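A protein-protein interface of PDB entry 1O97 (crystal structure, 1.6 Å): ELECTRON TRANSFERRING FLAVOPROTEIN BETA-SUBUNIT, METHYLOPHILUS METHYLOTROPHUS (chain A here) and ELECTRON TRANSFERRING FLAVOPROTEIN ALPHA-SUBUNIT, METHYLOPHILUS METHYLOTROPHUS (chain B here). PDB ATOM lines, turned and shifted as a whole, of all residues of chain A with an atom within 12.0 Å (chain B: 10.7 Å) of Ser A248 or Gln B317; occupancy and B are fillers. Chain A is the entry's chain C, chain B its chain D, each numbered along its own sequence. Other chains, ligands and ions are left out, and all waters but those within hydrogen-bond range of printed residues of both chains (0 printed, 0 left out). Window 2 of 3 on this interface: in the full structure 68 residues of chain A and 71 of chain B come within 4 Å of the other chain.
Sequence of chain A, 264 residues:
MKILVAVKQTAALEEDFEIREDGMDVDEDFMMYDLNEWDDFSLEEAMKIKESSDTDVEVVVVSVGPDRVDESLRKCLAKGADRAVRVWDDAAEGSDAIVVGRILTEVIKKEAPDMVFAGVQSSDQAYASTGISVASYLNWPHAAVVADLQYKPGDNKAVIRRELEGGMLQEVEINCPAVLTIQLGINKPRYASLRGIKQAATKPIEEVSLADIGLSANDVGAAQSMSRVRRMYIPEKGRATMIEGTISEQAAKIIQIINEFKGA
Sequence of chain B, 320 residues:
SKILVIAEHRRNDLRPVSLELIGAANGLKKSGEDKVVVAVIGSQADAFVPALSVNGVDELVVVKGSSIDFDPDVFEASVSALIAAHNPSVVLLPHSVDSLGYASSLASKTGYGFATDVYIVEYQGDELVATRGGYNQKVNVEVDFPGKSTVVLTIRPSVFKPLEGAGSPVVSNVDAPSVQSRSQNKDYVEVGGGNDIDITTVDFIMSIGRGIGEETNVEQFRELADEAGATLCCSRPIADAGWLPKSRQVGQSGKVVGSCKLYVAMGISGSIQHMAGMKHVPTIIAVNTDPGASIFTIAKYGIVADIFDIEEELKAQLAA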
ATOM      1  N   ILE A 243      17.220  -1.400 -18.538  1.00  0.00           N
ATOM      2  CA  ILE A 243      17.315  -2.690 -19.199  1.00  0.00           C
ATOM      3  C   ILE A 243      16.096  -2.901 -20.068  1.00  0.00           C
ATOM      4  O   ILE A 243      14.960  -2.984 -19.591  1.00  0.00           O
ATOM      5  CB  ILE A 243      17.484  -3.796 -18.201  1.00  0.00           C
ATOM      6  CG1 ILE A 243      18.571  -3.438 -17.178  1.00  0.00           C
ATOM      7  CG2 ILE A 243      17.728  -5.139 -18.958  1.00  0.00           C
ATOM      8  CD1 ILE A 243      18.635  -4.275 -16.009  1.00  0.00           C
ATOM      9  N   GLU A 244      16.345  -2.944 -21.361  1.00  0.00           N
ATOM     10  CA  GLU A 244      15.291  -3.132 -22.327  1.00  0.00           C
ATOM     11  C   GLU A 244      15.277  -4.616 -22.674  1.00  0.00           C
ATOM     12  O   GLU A 244      16.215  -5.387 -22.378  1.00  0.00           O
ATOM     13  CB  GLU A 244      15.505  -2.250 -23.576  1.00  0.00           C
ATOM     14  CG  GLU A 244      15.382  -0.751 -23.303  1.00  0.00           C
ATOM     15  CD  GLU A 244      15.432   0.142 -24.546  1.00  0.00           C
ATOM     16  OE1 GLU A 244      16.018  -0.263 -25.587  1.00  0.00           O
ATOM     17  OE2 GLU A 244      14.874   1.269 -24.485  1.00  0.00           O
ATOM     18  N   GLY A 245      14.208  -5.021 -23.307  1.00  0.00           N
ATOM     19  CA  GLY A 245      14.123  -6.404 -23.725  1.00  0.00           C
ATOM     20  C   GLY A 245      12.840  -7.002 -23.182  1.00  0.00           C
ATOM     21  O   GLY A 245      11.928  -6.283 -22.749  1.00  0.00           O
ATOM     22  N   THR A 246      12.777  -8.323 -23.252  1.00  0.00           N
ATOM     23  CA  THR A 246      11.609  -9.060 -22.773  1.00  0.00           C
ATOM     24  C   THR A 246      11.764  -9.299 -21.278  1.00  0.00           C
ATOM     25  O   THR A 246      12.860  -9.179 -20.720  1.00  0.00           O
ATOM     26  CB  THR A 246      11.520 -10.436 -23.497  1.00  0.00           C
ATOM     27  OG1 THR A 246      12.651 -11.231 -23.126  1.00  0.00           O
ATOM     28  CG2 THR A 246      11.628 -10.298 -24.991  1.00  0.00           C
ATOM     29  N   ILE A 247      10.669  -9.704 -20.622  1.00  0.00           N
ATOM     30  CA  ILE A 247      10.763 -10.140 -19.250  1.00  0.00           C
ATOM     31  C   ILE A 247      11.854 -11.148 -18.986  1.00  0.00           C
ATOM     32  O   ILE A 247      12.512 -11.036 -17.985  1.00  0.00           O
ATOM     33  CB  ILE A 247       9.382 -10.686 -18.761  1.00  0.00           C
ATOM     34  CG1 ILE A 247       8.342  -9.565 -18.795  1.00  0.00           C
ATOM     35  CG2 ILE A 247       9.513 -11.370 -17.402  1.00  0.00           C
ATOM     36  CD1 ILE A 247       8.473  -8.549 -17.643  1.00  0.00           C
ATOM     37  N   SER A 248      12.021 -12.157 -19.859  1.00  0.00           N
ATOM     38  CA  SER A 248      13.046 -13.180 -19.634  1.00  0.00           C
ATOM     39  C   SER A 248      14.479 -12.603 -19.599  1.00  0.00           C
ATOM     40  O   SER A 248      15.272 -12.991 -18.755  1.00  0.00           O
ATOM     41  CB  SER A 248      12.943 -14.313 -20.681  1.00  0.00           C
ATOM     42  N   GLU A 249      14.778 -11.670 -20.483  1.00  0.00           N
ATOM     43  CA  GLU A 249      16.125 -11.070 -20.477  1.00  0.00           C
ATOM     44  C   GLU A 249      16.348 -10.074 -19.349  1.00  0.00           C
ATOM     45  O   GLU A 249      17.417 -10.082 -18.727  1.00  0.00           O
ATOM     46  CB  GLU A 249      16.550 -10.491 -21.824  1.00  0.00           C
ATOM     47  CG  GLU A 249      15.557  -9.684 -22.623  1.00  0.00           C
ATOM     48  CD  GLU A 249      15.612 -10.090 -24.092  1.00  0.00           C
ATOM     49  OE1 GLU A 249      16.110 -11.204 -24.351  1.00  0.00           O
ATOM     50  OE2 GLU A 249      15.152  -9.322 -24.977  1.00  0.00           O
ATOM     51  N   GLN A 250      15.318  -9.259 -19.070  1.00  0.00           N
ATOM     52  CA  GLN A 250      15.323  -8.361 -17.909  1.00  0.00           C
ATOM     53  C   GLN A 250      15.579  -9.189 -16.664  1.00  0.00           C
ATOM     54  O   GLN A 250      16.402  -8.878 -15.815  1.00  0.00           O
ATOM     55  CB  GLN A 250      14.009  -7.560 -17.796  1.00  0.00           C
ATOM     56  CG  GLN A 250      13.841  -6.479 -18.842  1.00  0.00           C
ATOM     57  CD  GLN A 250      12.502  -5.812 -18.943  1.00  0.00           C
ATOM     58  OE1 GLN A 250      12.425  -4.630 -19.337  1.00  0.00           O
ATOM     59  NE2 GLN A 250      11.451  -6.547 -18.694  1.00  0.00           N
ATOM     60  N   ALA A 251      14.812 -10.279 -16.518  1.00  0.00           N
ATOM     61  CA  ALA A 251      15.071 -11.175 -15.399  1.00  0.00           C
ATOM     62  C   ALA A 251      16.463 -11.857 -15.464  1.00  0.00           C
ATOM     63  O   ALA A 251      17.092 -12.049 -14.430  1.00  0.00           O
ATOM     64  CB  ALA A 251      13.967 -12.226 -15.257  1.00  0.00           C
ATOM     65  N   ALA A 252      16.913 -12.219 -16.667  1.00  0.00           N
ATOM     66  CA  ALA A 252      18.282 -12.740 -16.848  1.00  0.00           C
ATOM     67  C   ALA A 252      19.330 -11.689 -16.397  1.00  0.00           C
ATOM     68  O   ALA A 252      20.138 -11.972 -15.483  1.00  0.00           O
ATOM     69  CB  ALA A 252      18.521 -13.180 -18.285  1.00  0.00           C
ATOM     70  N   LYS A 253      19.275 -10.487 -16.995  1.00  0.00           N
ATOM     71  CA  LYS A 253      20.018  -9.306 -16.442  1.00  0.00           C
ATOM     72  C   LYS A 253      20.089  -9.234 -14.908  1.00  0.00           C
ATOM     73  O   LYS A 253      21.179  -9.157 -14.341  1.00  0.00           O
ATOM     74  CB  LYS A 253      19.471  -8.008 -17.037  1.00  0.00           C
ATOM     75  CG  LYS A 253      20.482  -6.893 -17.175  1.00  0.00           C
ATOM     76  CD  LYS A 253      21.881  -7.379 -16.911  1.00  0.00           C
ATOM     77  CE  LYS A 253      22.870  -6.306 -17.206  1.00  0.00           C
ATOM     78  NZ  LYS A 253      24.060  -6.519 -16.335  1.00  0.00           N
ATOM     79  N   ILE A 254      18.936  -9.280 -14.221  1.00  0.00           N
ATOM     80  CA  ILE A 254      18.911  -9.254 -12.759  1.00  0.00           C
ATOM     81  C   ILE A 254      19.698 -10.393 -12.147  1.00  0.00           C
ATOM     82  O   ILE A 254      20.332 -10.236 -11.090  1.00  0.00           O
ATOM     83  CB  ILE A 254      17.436  -9.277 -12.196  1.00  0.00           C
ATOM     84  CG1 ILE A 254      16.678  -8.011 -12.576  1.00  0.00           C
ATOM     85  CG2 ILE A 254      17.414  -9.479 -10.677  1.00  0.00           C
ATOM     86  CD1 ILE A 254      15.230  -8.035 -12.087  1.00  0.00           C
ATOM     87  N   ILE A 255      19.641 -11.564 -12.786  1.00  0.00           N
ATOM     88  CA  ILE A 255      20.275 -12.740 -12.180  1.00  0.00           C
ATOM     89  C   ILE A 255      21.810 -12.630 -12.352  1.00  0.00           C
ATOM     90  O   ILE A 255      22.578 -12.900 -11.442  1.00  0.00           O
ATOM     91  CB  ILE A 255      19.731 -14.050 -12.793  1.00  0.00           C
ATOM     92  N   GLN A 256      22.214 -12.172 -13.527  1.00  0.00           N
ATOM     93  CA  GLN A 256      23.635 -11.852 -13.763  1.00  0.00           C
ATOM     94  C   GLN A 256      24.152 -10.817 -12.770  1.00  0.00           C
ATOM     95  O   GLN A 256      25.243 -10.973 -12.228  1.00  0.00           O
ATOM     96  CB  GLN A 256      23.883 -11.419 -15.218  1.00  0.00           C
ATOM     97  CG  GLN A 256      23.471 -12.497 -16.230  1.00  0.00           C
ATOM     98  CD  GLN A 256      24.158 -12.364 -17.595  1.00  0.00           C
ATOM     99  OE1 GLN A 256      24.217 -13.344 -18.371  1.00  0.00           O
ATOM    100  NE2 GLN A 256      24.675 -11.155 -17.893  1.00  0.00           N
ATOM    101  N   ILE A 257      23.341  -9.796 -12.479  1.00  0.00           N
ATOM    102  CA  ILE A 257      23.674  -8.870 -11.405  1.00  0.00           C
ATOM    103  C   ILE A 257      23.760  -9.537 -10.048  1.00  0.00           C
ATOM    104  O   ILE A 257      24.700  -9.254  -9.297  1.00  0.00           O
ATOM    105  CB  ILE A 257      22.715  -7.656 -11.368  1.00  0.00           C
ATOM    106  CG1 ILE A 257      22.811  -6.901 -12.687  1.00  0.00           C
ATOM    107  CG2 ILE A 257      23.059  -6.731 -10.182  1.00  0.00           C
ATOM    108  CD1 ILE A 257      21.602  -6.017 -13.034  1.00  0.00           C
ATOM    109  N   ILE A 258      22.810 -10.417  -9.709  1.00  0.00           N
ATOM    110  CA  ILE A 258      22.787 -11.035  -8.360  1.00  0.00           C
ATOM    111  C   ILE A 258      24.064 -11.843  -8.037  1.00  0.00           C
ATOM    112  O   ILE A 258      24.544 -11.849  -6.903  1.00  0.00           O
ATOM    113  CB  ILE A 258      21.515 -11.924  -8.120  1.00  0.00           C
ATOM    114  CG1 ILE A 258      20.257 -11.059  -7.922  1.00  0.00           C
ATOM    115  CG2 ILE A 258      21.698 -12.799  -6.879  1.00  0.00           C
ATOM    116  CD1 ILE A 258      18.951 -11.879  -7.726  1.00  0.00           C
ATOM    117  N   ASN A 259      24.590 -12.516  -9.044  1.00  0.00           N
ATOM    118  CA  ASN A 259      25.709 -13.438  -8.874  1.00  0.00           C
ATOM    119  C   ASN A 259      27.056 -12.736  -8.757  1.00  0.00           C
ATOM    120  O   ASN A 259      27.875 -13.097  -7.913  1.00  0.00           O
ATOM    121  CB  ASN A 259      25.758 -14.419 -10.050  1.00  0.00           C
ATOM    122  N   LEU B 224      10.225 -15.444  -3.368  1.00  0.00           N
ATOM    123  CA  LEU B 224      11.263 -14.976  -4.286  1.00  0.00           C
ATOM    124  C   LEU B 224      12.542 -14.654  -3.493  1.00  0.00           C
ATOM    125  O   LEU B 224      13.612 -15.054  -3.895  1.00  0.00           O
ATOM    126  CB  LEU B 224      10.802 -13.746  -5.061  1.00  0.00           C
ATOM    127  CG  LEU B 224      11.830 -13.123  -6.017  1.00  0.00           C
ATOM    128  CD1 LEU B 224      12.191 -14.056  -7.158  1.00  0.00           C
ATOM    129  CD2 LEU B 224      11.268 -11.830  -6.591  1.00  0.00           C
ATOM    130  N   GLU B 227      14.398 -17.886  -2.087  1.00  0.00           N
ATOM    131  CA  GLU B 227      15.110 -18.640  -3.114  1.00  0.00           C
ATOM    132  C   GLU B 227      16.321 -17.891  -3.647  1.00  0.00           C
ATOM    133  O   GLU B 227      17.298 -18.487  -4.132  1.00  0.00           O
ATOM    134  CB  GLU B 227      14.169 -18.946  -4.282  1.00  0.00           C
ATOM    135  N   ALA B 228      16.244 -16.570  -3.586  1.00  0.00           N
ATOM    136  CA  ALA B 228      17.372 -15.743  -4.005  1.00  0.00           C
ATOM    137  C   ALA B 228      18.471 -15.664  -2.972  1.00  0.00           C
ATOM    138  O   ALA B 228      19.618 -15.347  -3.292  1.00  0.00           O
ATOM    139  CB  ALA B 228      16.882 -14.308  -4.401  1.00  0.00           C
ATOM    140  N   ILE B 303      14.367  -1.292 -14.445  1.00  0.00           N
ATOM    141  CA  ILE B 303      13.553  -2.131 -15.306  1.00  0.00           C
ATOM    142  C   ILE B 303      12.134  -1.569 -15.216  1.00  0.00           C
ATOM    143  O   ILE B 303      11.541  -1.564 -14.128  1.00  0.00           O
ATOM    144  CB  ILE B 303      13.582  -3.562 -14.835  1.00  0.00           C
ATOM    145  CG1 ILE B 303      14.968  -4.158 -15.080  1.00  0.00           C
ATOM    146  CG2 ILE B 303      12.591  -4.389 -15.679  1.00  0.00           C
ATOM    147  CD1 ILE B 303      15.524  -4.901 -13.952  1.00  0.00           C
ATOM    148  N   ALA B 305       8.956  -2.511 -15.828  1.00  0.00           N
ATOM    149  CA  ALA B 305       8.144  -3.711 -16.081  1.00  0.00           C
ATOM    150  C   ALA B 305       7.277  -4.000 -14.886  1.00  0.00           C
ATOM    151  O   ALA B 305       7.526  -3.516 -13.778  1.00  0.00           O
ATOM    152  CB  ALA B 305       9.027  -4.924 -16.340  1.00  0.00           C
ATOM    153  N   ASP B 306       6.255  -4.829 -15.116  1.00  0.00           N
ATOM    154  CA  ASP B 306       5.391  -5.276 -14.053  1.00  0.00           C
ATOM    155  C   ASP B 306       6.106  -6.180 -13.066  1.00  0.00           C
ATOM    156  O   ASP B 306       6.742  -7.192 -13.380  1.00  0.00           O
ATOM    157  CB  ASP B 306       4.230  -6.007 -14.742  1.00  0.00           C
ATOM    158  CG  ASP B 306       3.206  -6.545 -13.734  1.00  0.00           C
ATOM    159  OD1 ASP B 306       3.312  -7.752 -13.399  1.00  0.00           O
ATOM    160  OD2 ASP B 306       2.284  -5.846 -13.250  1.00  0.00           O
ATOM    161  N   PHE B 308       5.048  -8.452 -10.984  1.00  0.00           N
ATOM    162  CA  PHE B 308       4.555  -9.811 -10.857  1.00  0.00           C
ATOM    163  C   PHE B 308       5.118 -10.667 -11.956  1.00  0.00           C
ATOM    164  O   PHE B 308       5.536 -11.793 -11.691  1.00  0.00           O
ATOM    165  CB  PHE B 308       3.016  -9.860 -10.804  1.00  0.00           C
ATOM    166  CG  PHE B 308       2.429  -8.893  -9.812  1.00  0.00           C
ATOM    167  CD1 PHE B 308       1.818  -7.706 -10.239  1.00  0.00           C
ATOM    168  CD2 PHE B 308       2.571  -9.130  -8.447  1.00  0.00           C
ATOM    169  CE1 PHE B 308       1.312  -6.759  -9.292  1.00  0.00           C
ATOM    170  CE2 PHE B 308       2.037  -8.190  -7.498  1.00  0.00           C
ATOM    171  CZ  PHE B 308       1.433  -7.043  -7.923  1.00  0.00           C
ATOM    172  N   ASP B 309       5.159 -10.105 -13.155  1.00  0.00           N
ATOM    173  CA  ASP B 309       5.798 -10.774 -14.332  1.00  0.00           C
ATOM    174  C   ASP B 309       7.297 -11.001 -14.118  1.00  0.00           C
ATOM    175  O   ASP B 309       7.814 -12.101 -14.353  1.00  0.00           O
ATOM    176  CB  ASP B 309       5.540  -9.991 -15.613  1.00  0.00           C
ATOM    177  CG  ASP B 309       4.089 -10.043 -16.054  1.00  0.00           C
ATOM    178  OD1 ASP B 309       3.295 -10.786 -15.436  1.00  0.00           O
ATOM    179  OD2 ASP B 309       3.643  -9.336 -16.986  1.00  0.00           O
ATOM    180  N   ILE B 310       8.013  -9.984 -13.632  1.00  0.00           N
ATOM    181  CA  ILE B 310       9.419 -10.189 -13.293  1.00  0.00           C
ATOM    182  C   ILE B 310       9.619 -11.225 -12.198  1.00  0.00           C
ATOM    183  O   ILE B 310      10.525 -12.075 -12.285  1.00  0.00           O
ATOM    184  CB  ILE B 310      10.085  -8.815 -12.884  1.00  0.00           C
ATOM    185  CG1 ILE B 310      10.119  -7.846 -14.085  1.00  0.00           C
ATOM    186  CG2 ILE B 310      11.415  -9.083 -12.147  1.00  0.00           C
ATOM    187  CD1 ILE B 310      11.232  -8.172 -15.144  1.00  0.00           C
ATOM    188  N   GLU B 311       8.807 -11.149 -11.145  1.00  0.00           N
ATOM    189  CA  GLU B 311       8.948 -12.039  -9.998  1.00  0.00           C
ATOM    190  C   GLU B 311       8.767 -13.508 -10.427  1.00  0.00           C
ATOM    191  O   GLU B 311       9.488 -14.399  -9.953  1.00  0.00           O
ATOM    192  CB  GLU B 311       7.928 -11.665  -8.909  1.00  0.00           C
ATOM    193  CG  GLU B 311       7.690 -12.731  -7.863  1.00  0.00           C
ATOM    194  CD  GLU B 311       6.489 -13.645  -8.166  1.00  0.00           C
ATOM    195  OE1 GLU B 311       5.619 -13.329  -9.027  1.00  0.00           O
ATOM    196  OE2 GLU B 311       6.424 -14.710  -7.513  1.00  0.00           O
ATOM    197  N   GLU B 312       7.790 -13.746 -11.298  1.00  0.00           N
ATOM    198  CA  GLU B 312       7.509 -15.125 -11.689  1.00  0.00           C
ATOM    199  C   GLU B 312       8.650 -15.652 -12.539  1.00  0.00           C
ATOM    200  O   GLU B 312       9.166 -16.735 -12.283  1.00  0.00           O
ATOM    201  CB  GLU B 312       6.116 -15.329 -12.301  1.00  0.00           C
ATOM    202  CG  GLU B 312       5.789 -14.617 -13.595  1.00  0.00           C
ATOM    203  CD  GLU B 312       4.646 -15.287 -14.373  1.00  0.00           C
ATOM    204  OE1 GLU B 312       4.405 -16.507 -14.180  1.00  0.00           O
ATOM    205  OE2 GLU B 312       3.980 -14.588 -15.188  1.00  0.00           O
ATOM    206  N   GLU B 313       9.093 -14.834 -13.483  1.00  0.00           N
ATOM    207  CA  GLU B 313      10.239 -15.192 -14.320  1.00  0.00           C
ATOM    208  C   GLU B 313      11.501 -15.386 -13.483  1.00  0.00           C
ATOM    209  O   GLU B 313      12.207 -16.395 -13.609  1.00  0.00           O
ATOM    210  CB  GLU B 313      10.435 -14.150 -15.411  1.00  0.00           C
ATOM    211  CG  GLU B 313      11.540 -14.457 -16.401  1.00  0.00           C
ATOM    212  CD  GLU B 313      11.200 -15.586 -17.358  1.00  0.00           C
ATOM    213  OE1 GLU B 313      10.113 -15.546 -17.995  1.00  0.00           O
ATOM    214  OE2 GLU B 313      12.048 -16.506 -17.468  1.00  0.00           O
ATOM    215  N   LEU B 314      11.777 -14.442 -12.592  1.00  0.00           N
ATOM    216  CA  LEU B 314      12.920 -14.559 -11.711  1.00  0.00           C
ATOM    217  C   LEU B 314      12.922 -15.907 -10.972  1.00  0.00           C
ATOM    218  O   LEU B 314      13.953 -16.592 -10.933  1.00  0.00           O
ATOM    219  CB  LEU B 314      12.908 -13.390 -10.727  1.00  0.00           C
ATOM    220  CG  LEU B 314      14.156 -12.589 -10.387  1.00  0.00           C
ATOM    221  CD1 LEU B 314      15.029 -12.357 -11.607  1.00  0.00           C
ATOM    222  CD2 LEU B 314      13.647 -11.298  -9.796  1.00  0.00           C
ATOM    223  N   LYS B 315      11.768 -16.291 -10.409  1.00  0.00           N
ATOM    224  CA  LYS B 315      11.638 -17.537  -9.637  1.00  0.00           C
ATOM    225  C   LYS B 315      11.843 -18.770 -10.513  1.00  0.00           C
ATOM    226  O   LYS B 315      12.390 -19.766 -10.044  1.00  0.00           O
ATOM    227  CB  LYS B 315      10.280 -17.632  -8.923  1.00  0.00           C
ATOM    228  N   ALA B 316      11.387 -18.681 -11.764  1.00  0.00           N
ATOM    229  CA  ALA B 316      11.568 -19.729 -12.776  1.00  0.00           C
ATOM    230  C   ALA B 316      13.056 -19.898 -13.100  1.00  0.00           C
ATOM    231  O   ALA B 316      13.604 -21.004 -13.002  1.00  0.00           O
ATOM    232  CB  ALA B 316      10.763 -19.392 -14.053  1.00  0.00           C
ATOM    233  N   GLN B 317      13.712 -18.798 -13.463  1.00  0.00           N
ATOM    234  CA  GLN B 317      15.136 -18.823 -13.785  1.00  0.00           C
ATOM    235  C   GLN B 317      16.008 -19.242 -12.612  1.00  0.00           C
ATOM    236  O   GLN B 317      17.066 -19.823 -12.832  1.00  0.00           O
ATOM    237  CB  GLN B 317      15.612 -17.487 -14.371  1.00  0.00           C
ATOM    238  CG  GLN B 317      14.987 -17.151 -15.719  1.00  0.00           C
ATOM    239  CD  GLN B 317      15.641 -15.983 -16.429  1.00  0.00           C
ATOM    240  OE1 GLN B 317      15.090 -15.463 -17.399  1.00  0.00           O
ATOM    241  NE2 GLN B 317      16.828 -15.591 -15.978  1.00  0.00           N
ATOM    242  N   LEU B 318      15.589 -18.977 -11.381  1.00  0.00           N
ATOM    243  CA  LEU B 318      16.374 -19.428 -10.225  1.00  0.00           C
ATOM    244  C   LEU B 318      16.153 -20.913  -9.940  1.00  0.00           C
ATOM    245  O   LEU B 318      17.018 -21.567  -9.355  1.00  0.00           O
ATOM    246  CB  LEU B 318      16.115 -18.580  -8.965  1.00  0.00           C
ATOM    247  CG  LEU B 318      16.511 -17.100  -8.992  1.00  0.00           C
ATOM    248  CD1 LEU B 318      16.055 -16.425  -7.704  1.00  0.00           C
ATOM    249  CD2 LEU B 318      18.012 -16.882  -9.252  1.00  0.00           C
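CD1 of Ile A243 touches CD1 of Ile B303, 3.8 Å away. CD1 of Ile A247 touches CB of Ala B305, 3.9 Å away. CG2 of Ile A247 touches CB of Glu B313 (3.5 Å). Glu B313 touches Ser A248. CD of Gln A250 touches CG2 of Ile B303 (3.6 Å). Ile B310 touches Gln A250 (CD1 to CB, 3.9 Å). Glu B313 touches Ala A251. O of Ala A251 touches CD1 of Leu B314, 3.5 Å away. Gln B317 touches Ala A251. Ile B303 touches Ile A254 (CD1 to CG1, 3.6 Å).
The backbone NH of Ser A248 lies close to the side-chain hydroxyl of Thr A246, 3.5 Å away. O of Ile A243 lies close to OE1 of Gln A250 (3.0 Å). OE1 of Gln B317 lies close to OE2 of Glu B313 (3.2 Å). The side-chain carboxylate (OD1) of Asp B306 is in hydrogen-bond range of the backbone NH (N) of Asp B309 (3.0 Å).
Of the printed residues of chain B, Ile A243 touches Ile B303. No residue of chain B comes within 4 Å of Glu A249. Of the printed residues of chain B, Gln A250 touches Ile B303 (3.6 Å), Ala B305 (3.7 Å) and Ile B310 (3.9 Å). Ala A251 touches just these residues of chain B: Glu B313, Leu B314 and Gln B317. Ile A255 touches none of the printed residues of chain B. Ile A258 touches none of the printed residues of chain B. Printed residues of chain A within 4 Å of Ile B303: Ile A243, Gln A250 and Ile A254. Printed residues of chain A within 4 Å of Ala B305: Ile A247 and Gln A250. Printed residues of chain A within 4 Å of Ile B310: Ile A247 (3.7 Å), Gln A250 (3.9 Å) and Ile A254 (3.96 Å). Glu B313 touches just these residues of chain A: Ile A247, Ser A248 and Ala A251. Of chain A, only Ala A251 (3.5 Å) and Ile A254 (3.9 Å) come within 4 Å of Leu B314. Gln B317 touches just these residues of chain A: Ser A248, Ala A251 and Ala A252. The nearest residue of chain B that does not touch Ser A248 is Ile B310 (6.2 Å). The nearest residue of chain A that does not touch Gln B317 is Ile A255 (4.6 Å).
Hydrophobic or aromatic side chains of chain B that line the printed part of chain A: Ile B303, Ala B305, Ile B310 and Leu B314. Printed residues of chain A that touch a printed residue of chain B: Ile A243, Ile A247, Ser A248, Gln A250, Ala A251, Ala A252 and Ile A254. Along chain A the printed residues that touch a printed residue of chain B span positions 243 to 254. Among the printed residues, no Asp or Glu carboxylate lies within 4 Å of a Lys or Arg side-chain nitrogen of the other chain.
The side-chain amide oxygen (OE1) of Gln B317 lies close to the backbone carbonyl oxygen (O) of Ser A248, 2.8 Å away. N of Ala A252 sits close to NE2 of Gln B317 (3.4 Å).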
